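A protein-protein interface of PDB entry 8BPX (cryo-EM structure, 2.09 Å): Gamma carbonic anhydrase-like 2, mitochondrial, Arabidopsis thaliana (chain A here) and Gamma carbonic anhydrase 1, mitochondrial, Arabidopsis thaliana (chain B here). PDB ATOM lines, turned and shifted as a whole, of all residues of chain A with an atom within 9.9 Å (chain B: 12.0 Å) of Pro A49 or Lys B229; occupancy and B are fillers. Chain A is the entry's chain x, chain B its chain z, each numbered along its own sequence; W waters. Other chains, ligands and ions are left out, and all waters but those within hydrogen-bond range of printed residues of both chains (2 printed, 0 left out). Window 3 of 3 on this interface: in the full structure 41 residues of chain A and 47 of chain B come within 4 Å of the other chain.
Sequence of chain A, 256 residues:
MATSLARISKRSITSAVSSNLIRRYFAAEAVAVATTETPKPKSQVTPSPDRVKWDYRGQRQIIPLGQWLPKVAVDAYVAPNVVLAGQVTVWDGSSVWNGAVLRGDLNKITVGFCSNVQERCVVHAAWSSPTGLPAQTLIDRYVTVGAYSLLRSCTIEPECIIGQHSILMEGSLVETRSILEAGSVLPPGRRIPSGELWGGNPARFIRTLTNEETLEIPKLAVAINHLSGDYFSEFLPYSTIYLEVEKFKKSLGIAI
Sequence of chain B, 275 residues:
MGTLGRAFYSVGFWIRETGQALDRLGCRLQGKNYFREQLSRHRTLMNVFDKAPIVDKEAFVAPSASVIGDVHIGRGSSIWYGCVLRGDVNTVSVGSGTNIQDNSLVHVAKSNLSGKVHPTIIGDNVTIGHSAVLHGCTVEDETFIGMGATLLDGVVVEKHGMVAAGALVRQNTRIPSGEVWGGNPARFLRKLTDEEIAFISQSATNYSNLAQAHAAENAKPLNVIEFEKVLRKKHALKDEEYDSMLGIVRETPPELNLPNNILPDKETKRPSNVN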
ATOM      1  N   THR A  46      16.822  25.637  -5.026  1.00  0.00           N
ATOM      2  CA  THR A  46      16.107  26.900  -5.098  1.00  0.00           C
ATOM      3  C   THR A  46      14.753  26.687  -5.757  1.00  0.00           C
ATOM      4  O   THR A  46      14.694  26.453  -6.974  1.00  0.00           O
ATOM      5  CB  THR A  46      16.924  27.947  -5.859  1.00  0.00           C
ATOM      6  OG1 THR A  46      16.301  29.231  -5.736  1.00  0.00           O
ATOM      7  CG2 THR A  46      17.086  27.570  -7.331  1.00  0.00           C
ATOM      8  N   PRO A  47      13.656  26.745  -5.012  1.00  0.00           N
ATOM      9  CA  PRO A  47      12.339  26.474  -5.592  1.00  0.00           C
ATOM     10  C   PRO A  47      11.816  27.655  -6.397  1.00  0.00           C
ATOM     11  O   PRO A  47      12.369  28.754  -6.386  1.00  0.00           O
ATOM     12  CB  PRO A  47      11.461  26.218  -4.363  1.00  0.00           C
ATOM     13  CG  PRO A  47      12.119  26.976  -3.278  1.00  0.00           C
ATOM     14  CD  PRO A  47      13.592  26.943  -3.556  1.00  0.00           C
ATOM     15  N   SER A  48      10.718  27.399  -7.104  1.00  0.00           N
ATOM     16  CA  SER A  48       9.986  28.410  -7.844  1.00  0.00           C
ATOM     17  C   SER A  48       8.665  28.704  -7.157  1.00  0.00           C
ATOM     18  O   SER A  48       7.916  27.770  -6.843  1.00  0.00           O
ATOM     19  CB  SER A  48       9.728  27.954  -9.282  1.00  0.00           C
ATOM     20  OG  SER A  48       8.736  26.946  -9.332  1.00  0.00           O
ATOM     21  N   PRO A  49       8.343  29.977  -6.912  1.00  0.00           N
ATOM     22  CA  PRO A  49       7.043  30.297  -6.301  1.00  0.00           C
ATOM     23  C   PRO A  49       5.855  29.954  -7.180  1.00  0.00           C
ATOM     24  O   PRO A  49       4.752  29.769  -6.653  1.00  0.00           O
ATOM     25  CB  PRO A  49       7.129  31.812  -6.049  1.00  0.00           C
ATOM     26  CG  PRO A  49       8.576  32.183  -6.273  1.00  0.00           C
ATOM     27  CD  PRO A  49       9.103  31.187  -7.252  1.00  0.00           C
ATOM     28  N   ASP A  50       6.039  29.856  -8.493  1.00  0.00           N
ATOM     29  CA  ASP A  50       4.926  29.686  -9.416  1.00  0.00           C
ATOM     30  C   ASP A  50       4.633  28.232  -9.773  1.00  0.00           C
ATOM     31  O   ASP A  50       3.751  27.989 -10.601  1.00  0.00           O
ATOM     32  CB  ASP A  50       5.184  30.479 -10.702  1.00  0.00           C
ATOM     33  CG  ASP A  50       6.434  30.029 -11.430  1.00  0.00           C
ATOM     34  OD1 ASP A  50       7.186  29.196 -10.884  1.00  0.00           O
ATOM     35  OD2 ASP A  50       6.666  30.512 -12.559  1.00  0.00           O
ATOM     36  N   ARG A  51       5.337  27.263  -9.192  1.00  0.00           N
ATOM     37  CA  ARG A  51       5.080  25.873  -9.548  1.00  0.00           C
ATOM     38  C   ARG A  51       3.707  25.443  -9.038  1.00  0.00           C
ATOM     39  O   ARG A  51       3.319  25.755  -7.909  1.00  0.00           O
ATOM     40  CB  ARG A  51       6.169  24.948  -8.995  1.00  0.00           C
ATOM     41  CG  ARG A  51       5.694  23.520  -8.709  1.00  0.00           C
ATOM     42  CD  ARG A  51       6.739  22.668  -8.004  1.00  0.00           C
ATOM     43  NE  ARG A  51       8.054  22.730  -8.632  1.00  0.00           N
ATOM     44  CZ  ARG A  51       8.397  22.076  -9.734  1.00  0.00           C
ATOM     45  NH1 ARG A  51       7.538  21.299 -10.374  1.00  0.00           N
ATOM     46  NH2 ARG A  51       9.635  22.197 -10.204  1.00  0.00           N
ATOM     47  N   VAL A  52       2.975  24.721  -9.882  1.00  0.00           N
ATOM     48  CA  VAL A  52       1.596  24.342  -9.589  1.00  0.00           C
ATOM     49  C   VAL A  52       1.591  23.226  -8.552  1.00  0.00           C
ATOM     50  O   VAL A  52       2.150  22.149  -8.781  1.00  0.00           O
ATOM     51  CB  VAL A  52       0.861  23.908 -10.865  1.00  0.00           C
ATOM     52  CG1 VAL A  52      -0.527  23.365 -10.527  1.00  0.00           C
ATOM     53  CG2 VAL A  52       0.778  25.060 -11.848  1.00  0.00           C
ATOM     54  N   LYS A  53       0.959  23.484  -7.411  1.00  0.00           N
ATOM     55  CA  LYS A  53       0.774  22.471  -6.382  1.00  0.00           C
ATOM     56  C   LYS A  53      -0.485  21.646  -6.618  1.00  0.00           C
ATOM     57  O   LYS A  53      -0.465  20.423  -6.455  1.00  0.00           O
ATOM     58  CB  LYS A  53       0.712  23.131  -5.004  1.00  0.00           C
ATOM     59  CG  LYS A  53       2.037  23.697  -4.534  1.00  0.00           C
ATOM     60  CD  LYS A  53       1.967  24.116  -3.084  1.00  0.00           C
ATOM     61  CE  LYS A  53       1.474  22.976  -2.214  1.00  0.00           C
ATOM     62  NZ  LYS A  53       2.586  22.311  -1.495  1.00  0.00           N
ATOM     63  N   TRP A  54      -1.584  22.298  -6.994  1.00  0.00           N
ATOM     64  CA  TRP A  54      -2.834  21.628  -7.328  1.00  0.00           C
ATOM     65  C   TRP A  54      -3.295  22.103  -8.696  1.00  0.00           C
ATOM     66  O   TRP A  54      -3.540  23.297  -8.891  1.00  0.00           O
ATOM     67  CB  TRP A  54      -3.913  21.899  -6.278  1.00  0.00           C
ATOM     68  CG  TRP A  54      -5.291  21.520  -6.729  1.00  0.00           C
ATOM     69  CD1 TRP A  54      -5.758  20.263  -6.965  1.00  0.00           C
ATOM     70  CD2 TRP A  54      -6.377  22.409  -7.016  1.00  0.00           C
ATOM     71  NE1 TRP A  54      -7.066  20.309  -7.371  1.00  0.00           N
ATOM     72  CE2 TRP A  54      -7.470  21.617  -7.414  1.00  0.00           C
ATOM     73  CE3 TRP A  54      -6.532  23.797  -6.977  1.00  0.00           C
ATOM     74  CZ2 TRP A  54      -8.697  22.166  -7.768  1.00  0.00           C
ATOM     75  CZ3 TRP A  54      -7.752  24.341  -7.324  1.00  0.00           C
ATOM     76  CH2 TRP A  54      -8.821  23.525  -7.715  1.00  0.00           C
ATOM     77  N   ASP A  55      -3.417  21.171  -9.635  1.00  0.00           N
ATOM     78  CA  ASP A  55      -3.893  21.453 -10.984  1.00  0.00           C
ATOM     79  C   ASP A  55      -5.342  20.985 -11.068  1.00  0.00           C
ATOM     80  O   ASP A  55      -5.619  19.785 -10.981  1.00  0.00           O
ATOM     81  CB  ASP A  55      -3.010  20.752 -12.017  1.00  0.00           C
ATOM     82  CG  ASP A  55      -3.305  21.182 -13.446  1.00  0.00           C
ATOM     83  OD1 ASP A  55      -4.468  21.497 -13.766  1.00  0.00           O
ATOM     84  OD2 ASP A  55      -2.364  21.186 -14.263  1.00  0.00           O
ATOM     85  N   TYR A  56      -6.267  21.936 -11.248  1.00  0.00           N
ATOM     86  CA  TYR A  56      -7.689  21.608 -11.245  1.00  0.00           C
ATOM     87  C   TYR A  56      -8.071  20.657 -12.370  1.00  0.00           C
ATOM     88  O   TYR A  56      -9.096  19.976 -12.268  1.00  0.00           O
ATOM     89  CB  TYR A  56      -8.536  22.884 -11.337  1.00  0.00           C
ATOM     90  CG  TYR A  56      -8.536  23.555 -12.696  1.00  0.00           C
ATOM     91  CD1 TYR A  56      -7.558  24.474 -13.035  1.00  0.00           C
ATOM     92  CD2 TYR A  56      -9.524  23.278 -13.638  1.00  0.00           C
ATOM     93  CE1 TYR A  56      -7.552  25.095 -14.266  1.00  0.00           C
ATOM     94  CE2 TYR A  56      -9.527  23.898 -14.878  1.00  0.00           C
ATOM     95  CZ  TYR A  56      -8.535  24.805 -15.185  1.00  0.00           C
ATOM     96  OH  TYR A  56      -8.517  25.431 -16.410  1.00  0.00           O
ATOM     97  N   ARG A  57      -7.276  20.595 -13.435  1.00  0.00           N
ATOM     98  CA  ARG A  57      -7.611  19.748 -14.571  1.00  0.00           C
ATOM     99  C   ARG A  57      -7.244  18.289 -14.350  1.00  0.00           C
ATOM    100  O   ARG A  57      -7.739  17.425 -15.080  1.00  0.00           O
ATOM    101  CB  ARG A  57      -6.916  20.268 -15.830  1.00  0.00           C
ATOM    102  CG  ARG A  57      -7.011  21.776 -16.002  1.00  0.00           C
ATOM    103  CD  ARG A  57      -6.003  22.291 -17.009  1.00  0.00           C
ATOM    104  NE  ARG A  57      -4.639  22.321 -16.491  1.00  0.00           N
ATOM    105  CZ  ARG A  57      -3.587  22.725 -17.192  1.00  0.00           C
ATOM    106  NH1 ARG A  57      -3.711  23.157 -18.436  1.00  0.00           N
ATOM    107  NH2 ARG A  57      -2.382  22.691 -16.633  1.00  0.00           N
ATOM    108  N   PHE A 248     -16.978  27.143 -10.181  1.00  0.00           N
ATOM    109  CA  PHE A 248     -15.806  27.455  -9.370  1.00  0.00           C
ATOM    110  C   PHE A 248     -15.215  28.800  -9.771  1.00  0.00           C
ATOM    111  O   PHE A 248     -14.757  29.566  -8.917  1.00  0.00           O
ATOM    112  CB  PHE A 248     -14.770  26.338  -9.517  1.00  0.00           C
ATOM    113  CG  PHE A 248     -13.737  26.298  -8.422  1.00  0.00           C
ATOM    114  CD1 PHE A 248     -12.633  27.131  -8.458  1.00  0.00           C
ATOM    115  CD2 PHE A 248     -13.858  25.403  -7.370  1.00  0.00           C
ATOM    116  CE1 PHE A 248     -11.677  27.085  -7.457  1.00  0.00           C
ATOM    117  CE2 PHE A 248     -12.903  25.354  -6.367  1.00  0.00           C
ATOM    118  CZ  PHE A 248     -11.813  26.198  -6.412  1.00  0.00           C
ATOM    119  N   LEU A 252     -15.453  32.870  -7.749  1.00  0.00           N
ATOM    120  CA  LEU A 252     -14.259  33.687  -7.574  1.00  0.00           C
ATOM    121  C   LEU A 252     -14.325  35.002  -8.334  1.00  0.00           C
ATOM    122  O   LEU A 252     -13.416  35.826  -8.196  1.00  0.00           O
ATOM    123  CB  LEU A 252     -13.014  32.909  -8.018  1.00  0.00           C
ATOM    124  CG  LEU A 252     -12.677  31.642  -7.232  1.00  0.00           C
ATOM    125  CD1 LEU A 252     -11.303  31.119  -7.625  1.00  0.00           C
ATOM    126  CD2 LEU A 252     -12.758  31.899  -5.739  1.00  0.00           C
ATOM    127  N   GLU B  37     -12.228  21.671 -22.926  1.00  0.00           N
ATOM    128  CA  GLU B  37     -11.072  21.486 -22.060  1.00  0.00           C
ATOM    129  C   GLU B  37     -10.908  20.016 -21.688  1.00  0.00           C
ATOM    130  O   GLU B  37     -11.877  19.341 -21.329  1.00  0.00           O
ATOM    131  CB  GLU B  37     -11.209  22.340 -20.799  1.00  0.00           C
ATOM    132  CG  GLU B  37     -10.013  22.251 -19.860  1.00  0.00           C
ATOM    133  CD  GLU B  37      -9.849  23.481 -18.986  1.00  0.00           C
ATOM    134  OE1 GLU B  37     -10.871  24.089 -18.609  1.00  0.00           O
ATOM    135  OE2 GLU B  37      -8.696  23.832 -18.664  1.00  0.00           O
ATOM    136  N   LEU B 222      -9.836  23.392  -1.610  1.00  0.00           N
ATOM    137  CA  LEU B 222      -8.910  23.579  -2.715  1.00  0.00           C
ATOM    138  C   LEU B 222      -8.476  25.038  -2.787  1.00  0.00           C
ATOM    139  O   LEU B 222      -9.309  25.948  -2.746  1.00  0.00           O
ATOM    140  CB  LEU B 222      -9.574  23.139  -4.019  1.00  0.00           C
ATOM    141  CG  LEU B 222     -10.064  21.687  -3.959  1.00  0.00           C
ATOM    142  CD1 LEU B 222     -10.807  21.285  -5.217  1.00  0.00           C
ATOM    143  CD2 LEU B 222      -8.905  20.734  -3.691  1.00  0.00           C
ATOM    144  N   ASN B 223      -7.166  25.258  -2.882  1.00  0.00           N
ATOM    145  CA  ASN B 223      -6.639  26.614  -2.848  1.00  0.00           C
ATOM    146  C   ASN B 223      -7.033  27.366  -4.113  1.00  0.00           C
ATOM    147  O   ASN B 223      -6.830  26.880  -5.229  1.00  0.00           O
ATOM    148  CB  ASN B 223      -5.117  26.593  -2.685  1.00  0.00           C
ATOM    149  CG  ASN B 223      -4.539  27.958  -2.364  1.00  0.00           C
ATOM    150  OD1 ASN B 223      -5.203  28.983  -2.517  1.00  0.00           O
ATOM    151  ND2 ASN B 223      -3.290  27.976  -1.911  1.00  0.00           N
ATOM    152  N   VAL B 224      -7.594  28.562  -3.931  1.00  0.00           N
ATOM    153  CA  VAL B 224      -8.029  29.362  -5.068  1.00  0.00           C
ATOM    154  C   VAL B 224      -6.872  30.102  -5.721  1.00  0.00           C
ATOM    155  O   VAL B 224      -6.968  30.467  -6.899  1.00  0.00           O
ATOM    156  CB  VAL B 224      -9.130  30.348  -4.640  1.00  0.00           C
ATOM    157  CG1 VAL B 224     -10.121  29.661  -3.720  1.00  0.00           C
ATOM    158  CG2 VAL B 224      -8.531  31.563  -3.964  1.00  0.00           C
ATOM    159  N   ILE B 225      -5.777  30.329  -4.989  1.00  0.00           N
ATOM    160  CA  ILE B 225      -4.601  30.960  -5.582  1.00  0.00           C
ATOM    161  C   ILE B 225      -3.992  30.061  -6.650  1.00  0.00           C
ATOM    162  O   ILE B 225      -3.602  30.531  -7.722  1.00  0.00           O
ATOM    163  CB  ILE B 225      -3.572  31.328  -4.494  1.00  0.00           C
ATOM    164  CG1 ILE B 225      -4.163  32.279  -3.443  1.00  0.00           C
ATOM    165  CG2 ILE B 225      -2.333  31.943  -5.119  1.00  0.00           C
ATOM    166  CD1 ILE B 225      -5.279  33.181  -3.933  1.00  0.00           C
ATOM    167  N   GLU B 226      -3.894  28.757  -6.377  1.00  0.00           N
ATOM    168  CA  GLU B 226      -3.389  27.835  -7.389  1.00  0.00           C
ATOM    169  C   GLU B 226      -4.302  27.809  -8.608  1.00  0.00           C
ATOM    170  O   GLU B 226      -3.826  27.773  -9.751  1.00  0.00           O
ATOM    171  CB  GLU B 226      -3.240  26.429  -6.804  1.00  0.00           C
ATOM    172  CG  GLU B 226      -2.339  26.341  -5.582  1.00  0.00           C
ATOM    173  CD  GLU B 226      -0.902  25.992  -5.930  1.00  0.00           C
ATOM    174  OE1 GLU B 226      -0.675  25.328  -6.963  1.00  0.00           O
ATOM    175  OE2 GLU B 226       0.004  26.383  -5.164  1.00  0.00           O
ATOM    176  N   PHE B 227      -5.617  27.829  -8.382  1.00  0.00           N
ATOM    177  CA  PHE B 227      -6.572  27.874  -9.485  1.00  0.00           C
ATOM    178  C   PHE B 227      -6.362  29.120 -10.339  1.00  0.00           C
ATOM    179  O   PHE B 227      -6.333  29.044 -11.572  1.00  0.00           O
ATOM    180  CB  PHE B 227      -7.998  27.826  -8.931  1.00  0.00           C
ATOM    181  CG  PHE B 227      -9.059  27.623  -9.978  1.00  0.00           C
ATOM    182  CD1 PHE B 227      -9.263  26.377 -10.547  1.00  0.00           C
ATOM    183  CD2 PHE B 227      -9.868  28.677 -10.378  1.00  0.00           C
ATOM    184  CE1 PHE B 227     -10.245  26.184 -11.503  1.00  0.00           C
ATOM    185  CE2 PHE B 227     -10.848  28.493 -11.334  1.00  0.00           C
ATOM    186  CZ  PHE B 227     -11.038  27.240 -11.898  1.00  0.00           C
ATOM    187  N   GLU B 228      -6.197  30.278  -9.693  1.00  0.00           N
ATOM    188  CA  GLU B 228      -5.977  31.519 -10.433  1.00  0.00           C
ATOM    189  C   GLU B 228      -4.636  31.521 -11.154  1.00  0.00           C
ATOM    190  O   GLU B 228      -4.523  32.083 -12.248  1.00  0.00           O
ATOM    191  CB  GLU B 228      -6.072  32.714  -9.488  1.00  0.00           C
ATOM    192  CG  GLU B 228      -7.475  32.995  -8.996  1.00  0.00           C
ATOM    193  CD  GLU B 228      -7.505  34.000  -7.861  1.00  0.00           C
ATOM    194  OE1 GLU B 228      -6.421  34.428  -7.415  1.00  0.00           O
ATOM    195  OE2 GLU B 228      -8.614  34.361  -7.415  1.00  0.00           O
ATOM    196  N   LYS B 229      -3.613  30.908 -10.557  1.00  0.00           N
ATOM    197  CA  LYS B 229      -2.320  30.789 -11.220  1.00  0.00           C
ATOM    198  C   LYS B 229      -2.417  29.931 -12.473  1.00  0.00           C
ATOM    199  O   LYS B 229      -1.809  30.246 -13.502  1.00  0.00           O
ATOM    200  CB  LYS B 229      -1.290  30.206 -10.253  1.00  0.00           C
ATOM    201  CG  LYS B 229      -0.215  31.187  -9.817  1.00  0.00           C
ATOM    202  CD  LYS B 229       0.565  30.658  -8.621  1.00  0.00           C
ATOM    203  CE  LYS B 229       0.784  29.154  -8.715  1.00  0.00           C
ATOM    204  NZ  LYS B 229       1.172  28.568  -7.406  1.00  0.00           N
ATOM    205  N   VAL B 230      -3.167  28.831 -12.402  1.00  0.00           N
ATOM    206  CA  VAL B 230      -3.325  27.981 -13.578  1.00  0.00           C
ATOM    207  C   VAL B 230      -4.160  28.687 -14.642  1.00  0.00           C
ATOM    208  O   VAL B 230      -3.874  28.587 -15.841  1.00  0.00           O
ATOM    209  CB  VAL B 230      -3.930  26.622 -13.182  1.00  0.00           C
ATOM    210  CG1 VAL B 230      -4.128  25.751 -14.408  1.00  0.00           C
ATOM    211  CG2 VAL B 230      -3.036  25.917 -12.179  1.00  0.00           C
ATOM    212  N   LEU B 231      -5.203  29.409 -14.225  1.00  0.00           N
ATOM    213  CA  LEU B 231      -6.050  30.114 -15.184  1.00  0.00           C
ATOM    214  C   LEU B 231      -5.280  31.202 -15.921  1.00  0.00           C
ATOM    215  O   LEU B 231      -5.424  31.360 -17.137  1.00  0.00           O
ATOM    216  CB  LEU B 231      -7.260  30.724 -14.479  1.00  0.00           C
ATOM    217  CG  LEU B 231      -8.381  29.807 -13.996  1.00  0.00           C
ATOM    218  CD1 LEU B 231      -9.681  30.591 -13.914  1.00  0.00           C
ATOM    219  CD2 LEU B 231      -8.531  28.598 -14.904  1.00  0.00           C
ATOM    220  N   ARG B 232      -4.461  31.963 -15.199  1.00  0.00           N
ATOM    221  CA  ARG B 232      -3.820  33.154 -15.736  1.00  0.00           C
ATOM    222  C   ARG B 232      -2.425  32.880 -16.293  1.00  0.00           C
ATOM    223  O   ARG B 232      -1.621  33.812 -16.407  1.00  0.00           O
ATOM    224  CB  ARG B 232      -3.756  34.239 -14.659  1.00  0.00           C
ATOM    225  CG  ARG B 232      -5.121  34.709 -14.173  1.00  0.00           C
ATOM    226  CD  ARG B 232      -4.998  35.648 -12.983  1.00  0.00           C
ATOM    227  NE  ARG B 232      -6.287  35.892 -12.347  1.00  0.00           N
ATOM    228  CZ  ARG B 232      -6.447  36.538 -11.199  1.00  0.00           C
ATOM    229  NH1 ARG B 232      -5.415  37.026 -10.531  1.00  0.00           N
ATOM    230  NH2 ARG B 232      -7.674  36.697 -10.709  1.00  0.00           N
ATOM    231  N   LYS B 233      -2.120  31.632 -16.633  1.00  0.00           N
ATOM    232  CA  LYS B 233      -0.816  31.310 -17.190  1.00  0.00           C
ATOM    233  C   LYS B 233      -0.681  31.859 -18.607  1.00  0.00           C
ATOM    234  O   LYS B 233      -1.662  31.997 -19.342  1.00  0.00           O
ATOM    235  CB  LYS B 233      -0.591  29.798 -17.191  1.00  0.00           C
ATOM    236  CG  LYS B 233       0.860  29.399 -17.390  1.00  0.00           C
ATOM    237  CD  LYS B 233       1.076  27.915 -17.181  1.00  0.00           C
ATOM    238  CE  LYS B 233       1.023  27.555 -15.706  1.00  0.00           C
ATOM    239  NZ  LYS B 233       1.924  28.417 -14.892  1.00  0.00           N
ATOM    240  N   LYS B 234       0.554  32.178 -18.983  1.00  0.00           N
ATOM    241  CA  LYS B 234       0.856  32.666 -20.322  1.00  0.00           C
ATOM    242  C   LYS B 234       2.176  32.087 -20.823  1.00  0.00           C
ATOM    243  O   LYS B 234       2.368  31.900 -22.023  1.00  0.00           O
ATOM    244  CB  LYS B 234       0.908  34.195 -20.341  1.00  0.00           C
ATOM    245  CG  LYS B 234      -0.455  34.867 -20.297  1.00  0.00           C
ATOM    246  CD  LYS B 234      -0.321  36.375 -20.175  1.00  0.00           C
ATOM    247  CE  LYS B 234      -1.684  37.052 -20.163  1.00  0.00           C
ATOM    248  NZ  LYS B 234      -1.569  38.530 -20.019  1.00  0.00           N
HETATM  249  O   HOH W   1     -10.765  26.471 -17.577  1.00  0.00           O
HETATM  250  O   HOH W   2      -6.455  22.966 -20.136  1.00  0.00           O
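Of the 14 printed residues of chain B, 9 touch a printed residue of chain A. Printed residues of chain B that touch a printed residue of chain A: Glu B37, Leu B222, Asn B223, Val B224, Glu B226, Phe B227, Lys B229, Val B230 and Leu B231. Hydrophobic or aromatic side chains of chain A within 4 Å of the printed part of chain B: Val A52, Trp A54, Tyr A56, Phe A248 and Leu A252. Along chain A the printed residues that touch a printed residue of chain B span positions 49 to 252.
The side-chain hydroxyl (OH) of Tyr A56 lies within hydrogen-bond range of the side-chain carboxylate (OE2) of Glu B37 (2.8 Å). The side-chain carboxylate (OE1) of Glu B226 sits at hydrogen-bond distance from the backbone NH (N) of Trp A54, at 3.2 Å. The backbone NH of Lys A53 is in hydrogen-bond range of the side-chain carboxylate of Glu B226 (2.5 Å).
Lys B229 touches just these residues of chain A: Pro A49, Asp A50 and Arg A51. No residue of chain B comes within 4 Å of Pro A47. No residue of chain B comes within 4 Å of Ser A48. Printed residues of chain B within 4 Å of Asp A50: Lys B229. Of the printed residues of chain B, Tyr A56 touches Glu B37 (2.8 Å), Phe B227 (3.4 Å), Val B230 (3.5 Å) and Leu B231 (3.5 Å). Of the printed residues of chain A, Asn B223 touches Trp A54. Of the printed residues of chain A, Leu B231 touches Tyr A56 (3.5 Å). The nearest residue of chain B that does not touch Pro A49 is Glu B226 (6.0 Å).
The side-chain amide oxygen of Asn B223 lies within hydrogen-bond range of the backbone NH of Ile B225, 2.9 Å away. The side-chain hydroxyl (OG) of Ser A48 sits close to the backbone NH (N) of Arg A51 (3.4 Å). The side-chain amino group of Lys B229 is in salt-bridge range of the side-chain carboxylate of Glu B226 (3.3 Å). The side-chain hydroxyl (OG) of Ser A48 is in hydrogen-bond range of the side-chain carboxylate (OD1) of Asp A50, 3.1 Å away. The guanidinium group (NH2) of Arg A57 is in salt-bridge range of the side-chain carboxylate (OD2) of Asp A55, at 2.8 Å.
Water W1 lies within hydrogen-bond range of OE1 of Glu B37 (2.6 Å) and OH of Tyr A56 (2.7 Å). Water W2 bridges OE2 of Glu B37 (2.8 Å) and NH1 of Arg A57 (3.2 Å).
Among the printed residues, pairs that only touch across the chains: Pro A49 with Lys B229 (3.9 Å), Asp A50 with Lys B229 (3.7 Å), Arg A51 with Lys B229 (3.6 Å), Val A52 with Glu B226 (3.5 Å), Val A52 with Val B230 (3.9 Å), Trp A54 with Leu B222 (3.4 Å), Trp A54 with Asn B223 (3.4 Å), Trp A54 with Phe B227 (3.8 Å), Tyr A56 with Phe B227 (3.4 Å), Tyr A56 with Val B230 (3.5 Å), Tyr A56 with Leu B231 (3.5 Å), Arg A57 with Glu B37 (3.5 Å), Phe A248 with Phe B227 (3.6 Å), Leu A252 with Val B224 (3.8 Å) and Leu A252 with Phe B227 (3.9 Å).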
